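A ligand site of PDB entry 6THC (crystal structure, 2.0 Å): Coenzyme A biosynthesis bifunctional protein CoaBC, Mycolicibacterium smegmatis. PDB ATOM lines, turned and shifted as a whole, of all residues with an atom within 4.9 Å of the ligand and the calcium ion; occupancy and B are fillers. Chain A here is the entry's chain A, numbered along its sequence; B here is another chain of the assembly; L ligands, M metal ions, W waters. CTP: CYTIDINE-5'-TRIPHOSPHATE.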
ATOM      1  N   MET A  98      -3.799  19.240  13.639  1.00  0.00           N
ATOM      2  CA  MET A  98      -3.055  18.326  14.517  1.00  0.00           C
ATOM      3  C   MET A  98      -3.892  18.081  15.758  1.00  0.00           C
ATOM      4  O   MET A  98      -3.665  18.665  16.828  1.00  0.00           O
ATOM      5  CB  MET A  98      -1.682  18.893  14.862  1.00  0.00           C
ATOM      6  CG  MET A  98      -0.652  18.771  13.738  1.00  0.00           C
ATOM      7  SD  MET A  98      -0.231  17.060  13.326  1.00  0.00           S
ATOM      8  CE  MET A  98       0.535  16.414  14.807  1.00  0.00           C
ATOM      9  N   ALA A  99      -4.873  17.175  15.635  1.00  0.00           N
ATOM     10  CA  ALA A  99      -5.692  16.804  16.789  1.00  0.00           C
ATOM     11  C   ALA A  99      -5.217  15.535  17.476  1.00  0.00           C
ATOM     12  O   ALA A  99      -5.826  15.138  18.465  1.00  0.00           O
ATOM     13  CB  ALA A  99      -7.161  16.635  16.378  1.00  0.00           C
ATOM     14  N   ALA A 100      -4.146  14.907  16.994  1.00  0.00           N
ATOM     15  CA  ALA A 100      -3.635  13.698  17.630  1.00  0.00           C
ATOM     16  C   ALA A 100      -2.971  14.032  18.971  1.00  0.00           C
ATOM     17  O   ALA A 100      -2.394  15.109  19.138  1.00  0.00           O
ATOM     18  CB  ALA A 100      -2.619  12.977  16.728  1.00  0.00           C
ATOM     19  N   VAL A 102      -0.033  13.197  20.620  1.00  0.00           N
ATOM     20  CA  VAL A 102       1.241  12.641  20.216  1.00  0.00           C
ATOM     21  C   VAL A 102       2.111  12.416  21.434  1.00  0.00           C
ATOM     22  O   VAL A 102       2.402  13.366  22.170  1.00  0.00           O
ATOM     23  CB  VAL A 102       1.937  13.568  19.207  1.00  0.00           C
ATOM     24  CG1 VAL A 102       3.285  12.980  18.786  1.00  0.00           C
ATOM     25  CG2 VAL A 102       1.035  13.821  17.989  1.00  0.00           C
ATOM     26  N   ALA A 103       2.590  11.188  21.625  1.00  0.00           N
ATOM     27  CA  ALA A 103       3.424  10.908  22.789  1.00  0.00           C
ATOM     28  C   ALA A 103       4.678  11.762  22.761  1.00  0.00           C
ATOM     29  O   ALA A 103       5.300  11.929  21.712  1.00  0.00           O
ATOM     30  CB  ALA A 103       3.807   9.430  22.837  1.00  0.00           C
ATOM     31  N   ASP A 104       5.056  12.324  23.914  1.00  0.00           N
ATOM     32  CA  ASP A 104       6.225  13.194  23.957  1.00  0.00           C
ATOM     33  C   ASP A 104       7.539  12.434  24.062  1.00  0.00           C
ATOM     34  O   ASP A 104       8.593  13.018  23.800  1.00  0.00           O
ATOM     35  CB  ASP A 104       6.106  14.164  25.121  1.00  0.00           C
ATOM     36  CG  ASP A 104       4.924  15.090  24.983  1.00  0.00           C
ATOM     37  OD1 ASP A 104       4.973  15.979  24.096  1.00  0.00           O
ATOM     38  OD2 ASP A 104       3.943  14.909  25.721  1.00  0.00           O
ATOM     39  N   ASN A 130      10.479  12.624  21.549  1.00  0.00           N
ATOM     40  CA  ASN A 130       9.904  12.559  20.219  1.00  0.00           C
ATOM     41  C   ASN A 130       9.889  13.937  19.579  1.00  0.00           C
ATOM     42  O   ASN A 130       9.775  14.954  20.258  1.00  0.00           O
ATOM     43  CB  ASN A 130       8.460  12.030  20.269  1.00  0.00           C
ATOM     44  CG  ASN A 130       8.406  10.544  20.526  1.00  0.00           C
ATOM     45  OD1 ASN A 130       9.277   9.803  20.105  1.00  0.00           O
ATOM     46  ND2 ASN A 130       7.361  10.097  21.232  1.00  0.00           N
ATOM     47  N   ASP A 131       9.971  13.965  18.243  1.00  0.00           N
ATOM     48  CA  ASP A 131       9.886  15.238  17.524  1.00  0.00           C
ATOM     49  C   ASP A 131       8.506  15.861  17.694  1.00  0.00           C
ATOM     50  O   ASP A 131       7.486  15.162  17.733  1.00  0.00           O
ATOM     51  CB  ASP A 131      10.164  15.025  16.033  1.00  0.00           C
ATOM     52  CG  ASP A 131      11.617  14.713  15.736  1.00  0.00           C
ATOM     53  OD1 ASP A 131      12.506  15.138  16.510  1.00  0.00           O
ATOM     54  OD2 ASP A 131      11.862  14.041  14.724  1.00  0.00           O
ATOM     55  N   ASP A 132       8.487  17.190  17.742  1.00  0.00           N
ATOM     56  CA  ASP A 132       7.251  17.976  17.761  1.00  0.00           C
ATOM     57  C   ASP A 132       6.775  18.134  16.310  1.00  0.00           C
ATOM     58  O   ASP A 132       7.383  18.877  15.532  1.00  0.00           O
ATOM     59  CB  ASP A 132       7.518  19.325  18.428  1.00  0.00           C
ATOM     60  CG  ASP A 132       6.252  20.132  18.656  1.00  0.00           C
ATOM     61  OD1 ASP A 132       5.225  19.846  18.009  1.00  0.00           O
ATOM     62  OD2 ASP A 132       6.290  21.055  19.510  1.00  0.00           O
ATOM     63  N   VAL A 133       5.697  17.436  15.943  1.00  0.00           N
ATOM     64  CA  VAL A 133       5.303  17.446  14.535  1.00  0.00           C
ATOM     65  C   VAL A 133       4.656  18.776  14.166  1.00  0.00           C
ATOM     66  O   VAL A 133       4.929  19.333  13.088  1.00  0.00           O
ATOM     67  CB  VAL A 133       4.372  16.244  14.241  1.00  0.00           C
ATOM     68  CG1 VAL A 133       3.973  16.231  12.781  1.00  0.00           C
ATOM     69  CG2 VAL A 133       5.086  14.923  14.583  1.00  0.00           C
ATOM     70  N   LEU A 134       3.832  19.324  15.054  1.00  0.00           N
ATOM     71  CA  LEU A 134       3.188  20.612  14.823  1.00  0.00           C
ATOM     72  C   LEU A 134       4.221  21.730  14.640  1.00  0.00           C
ATOM     73  O   LEU A 134       4.131  22.529  13.702  1.00  0.00           O
ATOM     74  CB  LEU A 134       2.253  20.950  16.003  1.00  0.00           C
ATOM     75  CG  LEU A 134       1.510  22.298  16.045  1.00  0.00           C
ATOM     76  CD1 LEU A 134       0.629  22.512  14.834  1.00  0.00           C
ATOM     77  CD2 LEU A 134       0.650  22.469  17.298  1.00  0.00           C
ATOM     78  N   GLY A 154      -3.428  23.565  15.818  1.00  0.00           N
ATOM     79  CA  GLY A 154      -3.123  22.667  16.904  1.00  0.00           C
ATOM     80  C   GLY A 154      -4.226  22.579  17.936  1.00  0.00           C
ATOM     81  O   GLY A 154      -5.157  23.390  17.947  1.00  0.00           O
ATOM     82  N   PHE A 155      -4.133  21.561  18.800  1.00  0.00           N
ATOM     83  CA  PHE A 155      -5.094  21.307  19.866  1.00  0.00           C
ATOM     84  C   PHE A 155      -4.329  21.222  21.184  1.00  0.00           C
ATOM     85  O   PHE A 155      -3.183  20.790  21.214  1.00  0.00           O
ATOM     86  CB  PHE A 155      -5.835  19.990  19.647  1.00  0.00           C
ATOM     87  CG  PHE A 155      -6.929  20.055  18.633  1.00  0.00           C
ATOM     88  CD1 PHE A 155      -6.660  20.374  17.306  1.00  0.00           C
ATOM     89  CD2 PHE A 155      -8.234  19.802  19.002  1.00  0.00           C
ATOM     90  CE1 PHE A 155      -7.685  20.436  16.375  1.00  0.00           C
ATOM     91  CE2 PHE A 155      -9.250  19.854  18.069  1.00  0.00           C
ATOM     92  CZ  PHE A 155      -8.985  20.175  16.766  1.00  0.00           C
ATOM     93  N   ALA A 156      -4.967  21.616  22.275  1.00  0.00           N
ATOM     94  CA  ALA A 156      -4.288  21.535  23.553  1.00  0.00           C
ATOM     95  C   ALA A 156      -5.346  21.384  24.641  1.00  0.00           C
ATOM     96  O   ALA A 156      -6.428  21.971  24.546  1.00  0.00           O
ATOM     97  CB  ALA A 156      -3.441  22.786  23.802  1.00  0.00           C
ATOM     98  N   ALA A 157      -5.022  20.590  25.657  1.00  0.00           N
ATOM     99  CA  ALA A 157      -5.788  20.514  26.891  1.00  0.00           C
ATOM    100  C   ALA A 157      -4.973  21.227  27.962  1.00  0.00           C
ATOM    101  O   ALA A 157      -3.823  20.886  28.204  1.00  0.00           O
ATOM    102  CB  ALA A 157      -6.078  19.064  27.299  1.00  0.00           C
ATOM    103  N   GLU A 158      -5.566  22.251  28.570  1.00  0.00           N
ATOM    104  CA  GLU A 158      -4.868  23.086  29.532  1.00  0.00           C
ATOM    105  C   GLU A 158      -5.651  23.157  30.830  1.00  0.00           C
ATOM    106  O   GLU A 158      -6.874  23.056  30.846  1.00  0.00           O
ATOM    107  CB  GLU A 158      -4.659  24.519  28.995  1.00  0.00           C
ATOM    108  CG  GLU A 158      -3.843  24.595  27.707  1.00  0.00           C
ATOM    109  CD  GLU A 158      -2.384  24.223  27.910  1.00  0.00           C
ATOM    110  OE1 GLU A 158      -1.687  24.014  26.895  1.00  0.00           O
ATOM    111  OE2 GLU A 158      -1.941  24.129  29.081  1.00  0.00           O
ATOM    112  N   LYS A 173       1.129  28.566  24.970  1.00  0.00           N
ATOM    113  CA  LYS A 173       1.238  27.442  24.056  1.00  0.00           C
ATOM    114  C   LYS A 173       1.090  27.908  22.611  1.00  0.00           C
ATOM    115  O   LYS A 173       1.868  27.502  21.732  1.00  0.00           O
ATOM    116  CB  LYS A 173       0.146  26.415  24.360  1.00  0.00           C
ATOM    117  CG  LYS A 173       0.516  24.961  24.078  1.00  0.00           C
ATOM    118  CD  LYS A 173       1.190  24.452  25.336  1.00  0.00           C
ATOM    119  CE  LYS A 173       1.356  22.989  25.387  1.00  0.00           C
ATOM    120  NZ  LYS A 173       0.237  22.366  26.129  1.00  0.00           N
ATOM    121  N   ARG A 176       4.244  29.643  21.693  1.00  0.00           N
ATOM    122  CA  ARG A 176       5.395  28.763  21.503  1.00  0.00           C
ATOM    123  C   ARG A 176       5.263  27.910  20.250  1.00  0.00           C
ATOM    124  O   ARG A 176       6.263  27.664  19.559  1.00  0.00           O
ATOM    125  CB  ARG A 176       5.589  27.839  22.699  1.00  0.00           C
ATOM    126  CG  ARG A 176       6.313  28.479  23.874  1.00  0.00           C
ATOM    127  CD  ARG A 176       6.777  27.443  24.900  1.00  0.00           C
ATOM    128  NE  ARG A 176       5.829  26.352  25.095  1.00  0.00           N
ATOM    129  CZ  ARG A 176       4.865  26.338  26.009  1.00  0.00           C
ATOM    130  NH1 ARG A 176       4.714  27.362  26.840  1.00  0.00           N
ATOM    131  NH2 ARG A 176       4.056  25.284  26.103  1.00  0.00           N
ATOM    132  N   LYS A 177       4.063  27.404  19.957  1.00  0.00           N
ATOM    133  CA  LYS A 177       3.853  26.571  18.779  1.00  0.00           C
ATOM    134  C   LYS A 177       3.919  27.398  17.498  1.00  0.00           C
ATOM    135  O   LYS A 177       4.460  26.948  16.483  1.00  0.00           O
ATOM    136  CB  LYS A 177       2.501  25.859  18.853  1.00  0.00           C
ATOM    137  CG  LYS A 177       2.372  24.837  19.971  1.00  0.00           C
ATOM    138  CD  LYS A 177       3.557  23.888  19.961  1.00  0.00           C
ATOM    139  CE  LYS A 177       3.351  22.699  20.888  1.00  0.00           C
ATOM    140  NZ  LYS A 177       3.752  21.400  20.202  1.00  0.00           N
ATOM    141  N   ARG B  30      -1.471   9.372  30.798  1.00  0.00           N
ATOM    142  CA  ARG B  30      -0.579   8.348  30.217  1.00  0.00           C
ATOM    143  C   ARG B  30      -0.540   7.084  31.078  1.00  0.00           C
ATOM    144  O   ARG B  30      -0.698   7.212  32.270  1.00  0.00           O
ATOM    145  CB  ARG B  30       0.824   8.929  30.075  1.00  0.00           C
ATOM    146  CG  ARG B  30       0.912  10.017  29.035  1.00  0.00           C
ATOM    147  CD  ARG B  30       1.695  11.161  29.605  1.00  0.00           C
ATOM    148  NE  ARG B  30       2.124  12.132  28.625  1.00  0.00           N
ATOM    149  CZ  ARG B  30       2.520  13.337  28.955  1.00  0.00           C
ATOM    150  NH1 ARG B  30       2.510  13.682  30.224  1.00  0.00           N
ATOM    151  NH2 ARG B  30       2.907  14.198  28.042  1.00  0.00           N
ATOM    152  N   LYS B 114      -0.656  16.217  34.885  1.00  0.00           N
ATOM    153  CA  LYS B 114      -0.014  15.838  33.630  1.00  0.00           C
ATOM    154  C   LYS B 114       1.445  16.280  33.663  1.00  0.00           C
ATOM    155  O   LYS B 114       1.744  17.452  33.884  1.00  0.00           O
ATOM    156  CB  LYS B 114      -0.744  16.465  32.441  1.00  0.00           C
ATOM    157  CG  LYS B 114       0.019  16.363  31.122  1.00  0.00           C
ATOM    158  CD  LYS B 114      -0.666  17.150  29.994  1.00  0.00           C
ATOM    159  CE  LYS B 114       0.374  17.799  29.077  1.00  0.00           C
ATOM    160  NZ  LYS B 114      -0.243  18.501  27.891  1.00  0.00           N
ATOM    161  N   ILE B 115       2.360  15.329  33.465  1.00  0.00           N
ATOM    162  CA  ILE B 115       3.779  15.642  33.501  1.00  0.00           C
ATOM    163  C   ILE B 115       4.148  16.483  32.288  1.00  0.00           C
ATOM    164  O   ILE B 115       3.924  16.072  31.144  1.00  0.00           O
ATOM    165  CB  ILE B 115       4.614  14.359  33.565  1.00  0.00           C
ATOM    166  CG1 ILE B 115       4.508  13.737  34.950  1.00  0.00           C
ATOM    167  CG2 ILE B 115       6.074  14.641  33.244  1.00  0.00           C
ATOM    168  CD1 ILE B 115       4.573  12.252  34.927  1.00  0.00           C
ATOM    169  N   LYS B 116       4.700  17.665  32.531  1.00  0.00           N
ATOM    170  CA  LYS B 116       5.065  18.591  31.465  1.00  0.00           C
ATOM    171  C   LYS B 116       6.442  18.262  30.928  1.00  0.00           C
ATOM    172  O   LYS B 116       7.361  17.946  31.694  1.00  0.00           O
ATOM    173  CB  LYS B 116       5.044  20.038  31.971  1.00  0.00           C
ATOM    174  CG  LYS B 116       3.796  20.431  32.765  1.00  0.00           C
ATOM    175  CD  LYS B 116       2.893  21.376  31.969  1.00  0.00           C
ATOM    176  CE  LYS B 116       1.815  20.601  31.227  1.00  0.00           C
ATOM    177  NZ  LYS B 116       1.053  21.466  30.281  1.00  0.00           N
ATOM    178  N   LYS B 117       6.593  18.331  29.613  1.00  0.00           N
ATOM    179  CA  LYS B 117       7.901  18.182  29.002  1.00  0.00           C
ATOM    180  C   LYS B 117       8.754  19.416  29.278  1.00  0.00           C
ATOM    181  O   LYS B 117       8.288  20.551  29.200  1.00  0.00           O
ATOM    182  CB  LYS B 117       7.767  17.964  27.494  1.00  0.00           C
ATOM    183  CG  LYS B 117       6.689  16.982  27.120  1.00  0.00           C
HETATM  184  N1  CTP L   1       2.203  17.709  19.087  1.00  0.00           N
HETATM  185  C2  CTP L   1       3.044  17.354  18.043  1.00  0.00           C
HETATM  186  N3  CTP L   1       4.146  16.619  18.295  1.00  0.00           N
HETATM  187  C4  CTP L   1       4.427  16.244  19.536  1.00  0.00           C
HETATM  188  C5  CTP L   1       3.584  16.601  20.622  1.00  0.00           C
HETATM  189  C6  CTP L   1       2.503  17.334  20.360  1.00  0.00           C
HETATM  190  O2  CTP L   1       2.764  17.742  16.913  1.00  0.00           O
HETATM  191  N4  CTP L   1       5.507  15.516  19.751  1.00  0.00           N
HETATM  192  C1' CTP L   1       1.023  18.551  18.784  1.00  0.00           C
HETATM  193  C2' CTP L   1      -0.304  17.951  19.242  1.00  0.00           C
HETATM  194  O2' CTP L   1      -0.864  17.231  18.187  1.00  0.00           O
HETATM  195  C3' CTP L   1      -1.128  19.199  19.585  1.00  0.00           C
HETATM  196  C4' CTP L   1      -0.082  20.248  19.941  1.00  0.00           C
HETATM  197  O4' CTP L   1       1.191  19.765  19.445  1.00  0.00           O
HETATM  198  O3' CTP L   1      -1.908  19.675  18.517  1.00  0.00           O
HETATM  199  C5' CTP L   1       0.037  20.631  21.390  1.00  0.00           C
HETATM  200  O5' CTP L   1       0.245  19.477  22.176  1.00  0.00           O
HETATM  201  PA  CTP L   1       0.414  19.590  23.735  1.00  0.00           P
HETATM  202  O1A CTP L   1       0.382  18.244  24.272  1.00  0.00           O
HETATM  203  O2A CTP L   1      -0.618  20.466  24.305  1.00  0.00           O
HETATM  204  O3A CTP L   1       1.782  20.314  23.933  1.00  0.00           O
HETATM  205  PB  CTP L   1       3.306  20.055  24.193  1.00  0.00           P
HETATM  206  O1B CTP L   1       3.708  18.752  23.817  1.00  0.00           O
HETATM  207  O2B CTP L   1       4.013  21.146  23.561  1.00  0.00           O
HETATM  208  O3B CTP L   1       3.474  20.291  25.755  1.00  0.00           O
HETATM  209  PG  CTP L   1       3.059  19.737  27.162  1.00  0.00           P
HETATM  210  O1G CTP L   1       4.244  19.864  27.975  1.00  0.00           O
HETATM  211  O2G CTP L   1       2.647  18.381  27.088  1.00  0.00           O
HETATM  212  O3G CTP L   1       1.988  20.609  27.609  1.00  0.00           O
HETATM  213 CA    CA M   1       2.410  16.848  24.984  1.00  0.00          CA
HETATM  214  O   HOH W   1       0.604  15.790  26.277  1.00  0.00           O
HETATM  215  O   HOH W   2       1.540  15.519  23.273  1.00  0.00           O
HETATM  216  O   HOH W   3      -2.331  19.593  25.810  1.00  0.00           O
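Water W2 is bound to the calcium ion, 2.3 Å away.
The calcium ion is bound by water W1.
The calcium ion is bound by O1A of the ligand (2.6 Å).
OD2 of Asp 104 is bound to the calcium ion (2.6 Å).
An oxygen (O1B) of the ligand binds the calcium ion, at 2.6 Å.
An oxygen (O2G) of the ligand binds the calcium ion (2.6 Å).
The side-chain carboxylate (OD1) of Asp 104 binds the calcium ion, at 2.8 Å.
N3 of the ligand sits close to OD1 of Asp 132 (3.4 Å).
Merely in contact with the ligand: Val 102 (3.5 Å), Gly 154 (3.6 Å) and Ala 156 (3.7 Å).
Hydrophobic or aromatic side chains within 4 Å of the ligand: Met 98, Val 102, Val 133, Leu 134 and Ala 156.
Within 4 Å of the ligand: Met 98, Ala 100, Val 102, Asp 104, Asp 131, Asp 132, Val 133, Leu 134, Gly 154, Phe 155, Ala 156, Lys 173, Lys 177, Lys 114 of chain B, Lys 116 of chain B and Lys 117 of chain B.
Water W1 lies within hydrogen-bond range of NZ of Lys 114 of chain B and NH2 of Arg 30 of chain B.
Water W3 lies within hydrogen-bond range of O2A of the ligand, N of Ala 157 and NZ of Lys 114 of chain B.
The nearest printed residue that does not touch the calcium ion is Arg 30 of chain B (4.1 Å).
The backbone carbonyl oxygen (O) of Met 98 sits at hydrogen-bond distance from an oxygen (O3') of the ligand.
N of Leu 134 is in hydrogen-bond range of O2 of the ligand, at 2.7 Å.
An oxygen (O2A) of the ligand lies within salt-bridge range of the side-chain amino group (NZ) of Lys 173, 2.8 Å away.
The backbone carbonyl oxygen (O) of Ala 100 sits at hydrogen-bond distance from an oxygen (O2') of the ligand (2.8 Å).
O of Asp 131 lies within hydrogen-bond range of N4 of the ligand (2.8 Å).
An oxygen (O3') of the ligand lies within hydrogen-bond range of the backbone NH (N) of Phe 155 (2.9 Å).
An oxygen (O3') of the ligand sits close to the backbone carbonyl oxygen (O) of Phe 155, at 3.2 Å.
The backbone NH of Val 133 is in hydrogen-bond range of a nitrogen (N3) of the ligand (2.9 Å).
O3G of the ligand lies within salt-bridge range of NZ of Lys 116 of chain B, 3.0 Å away.
NZ of Lys 114 of chain B is in salt-bridge range of O3G of the ligand, at 3.1 Å.
The side-chain amino group (NZ) of Lys 177 lies within salt-bridge range of an oxygen (O2B) of the ligand (3.4 Å).
The backbone NH (N) of Lys 117 of chain B is in hydrogen-bond range of an oxygen (O1G) of the ligand (3.2 Å).
The guanidinium group (NH2) of Arg 30 of chain B lies close to the side-chain carboxylate (OD2) of Asp 104 (2.6 Å).
The backbone NH (N) of Asn 130 sits at hydrogen-bond distance from the backbone carbonyl oxygen (O) of Asp 104.
The backbone NH (N) of Leu 134 sits at hydrogen-bond distance from the side-chain carboxylate (OD1) of Asp 132, at 3.3 Å.
NZ of Lys 173 is in salt-bridge range of OE1 of Glu 158, 2.6 Å away.
The side-chain amino group of Lys 177 lies within salt-bridge range of the side-chain carboxylate of Asp 132 (2.7 Å).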
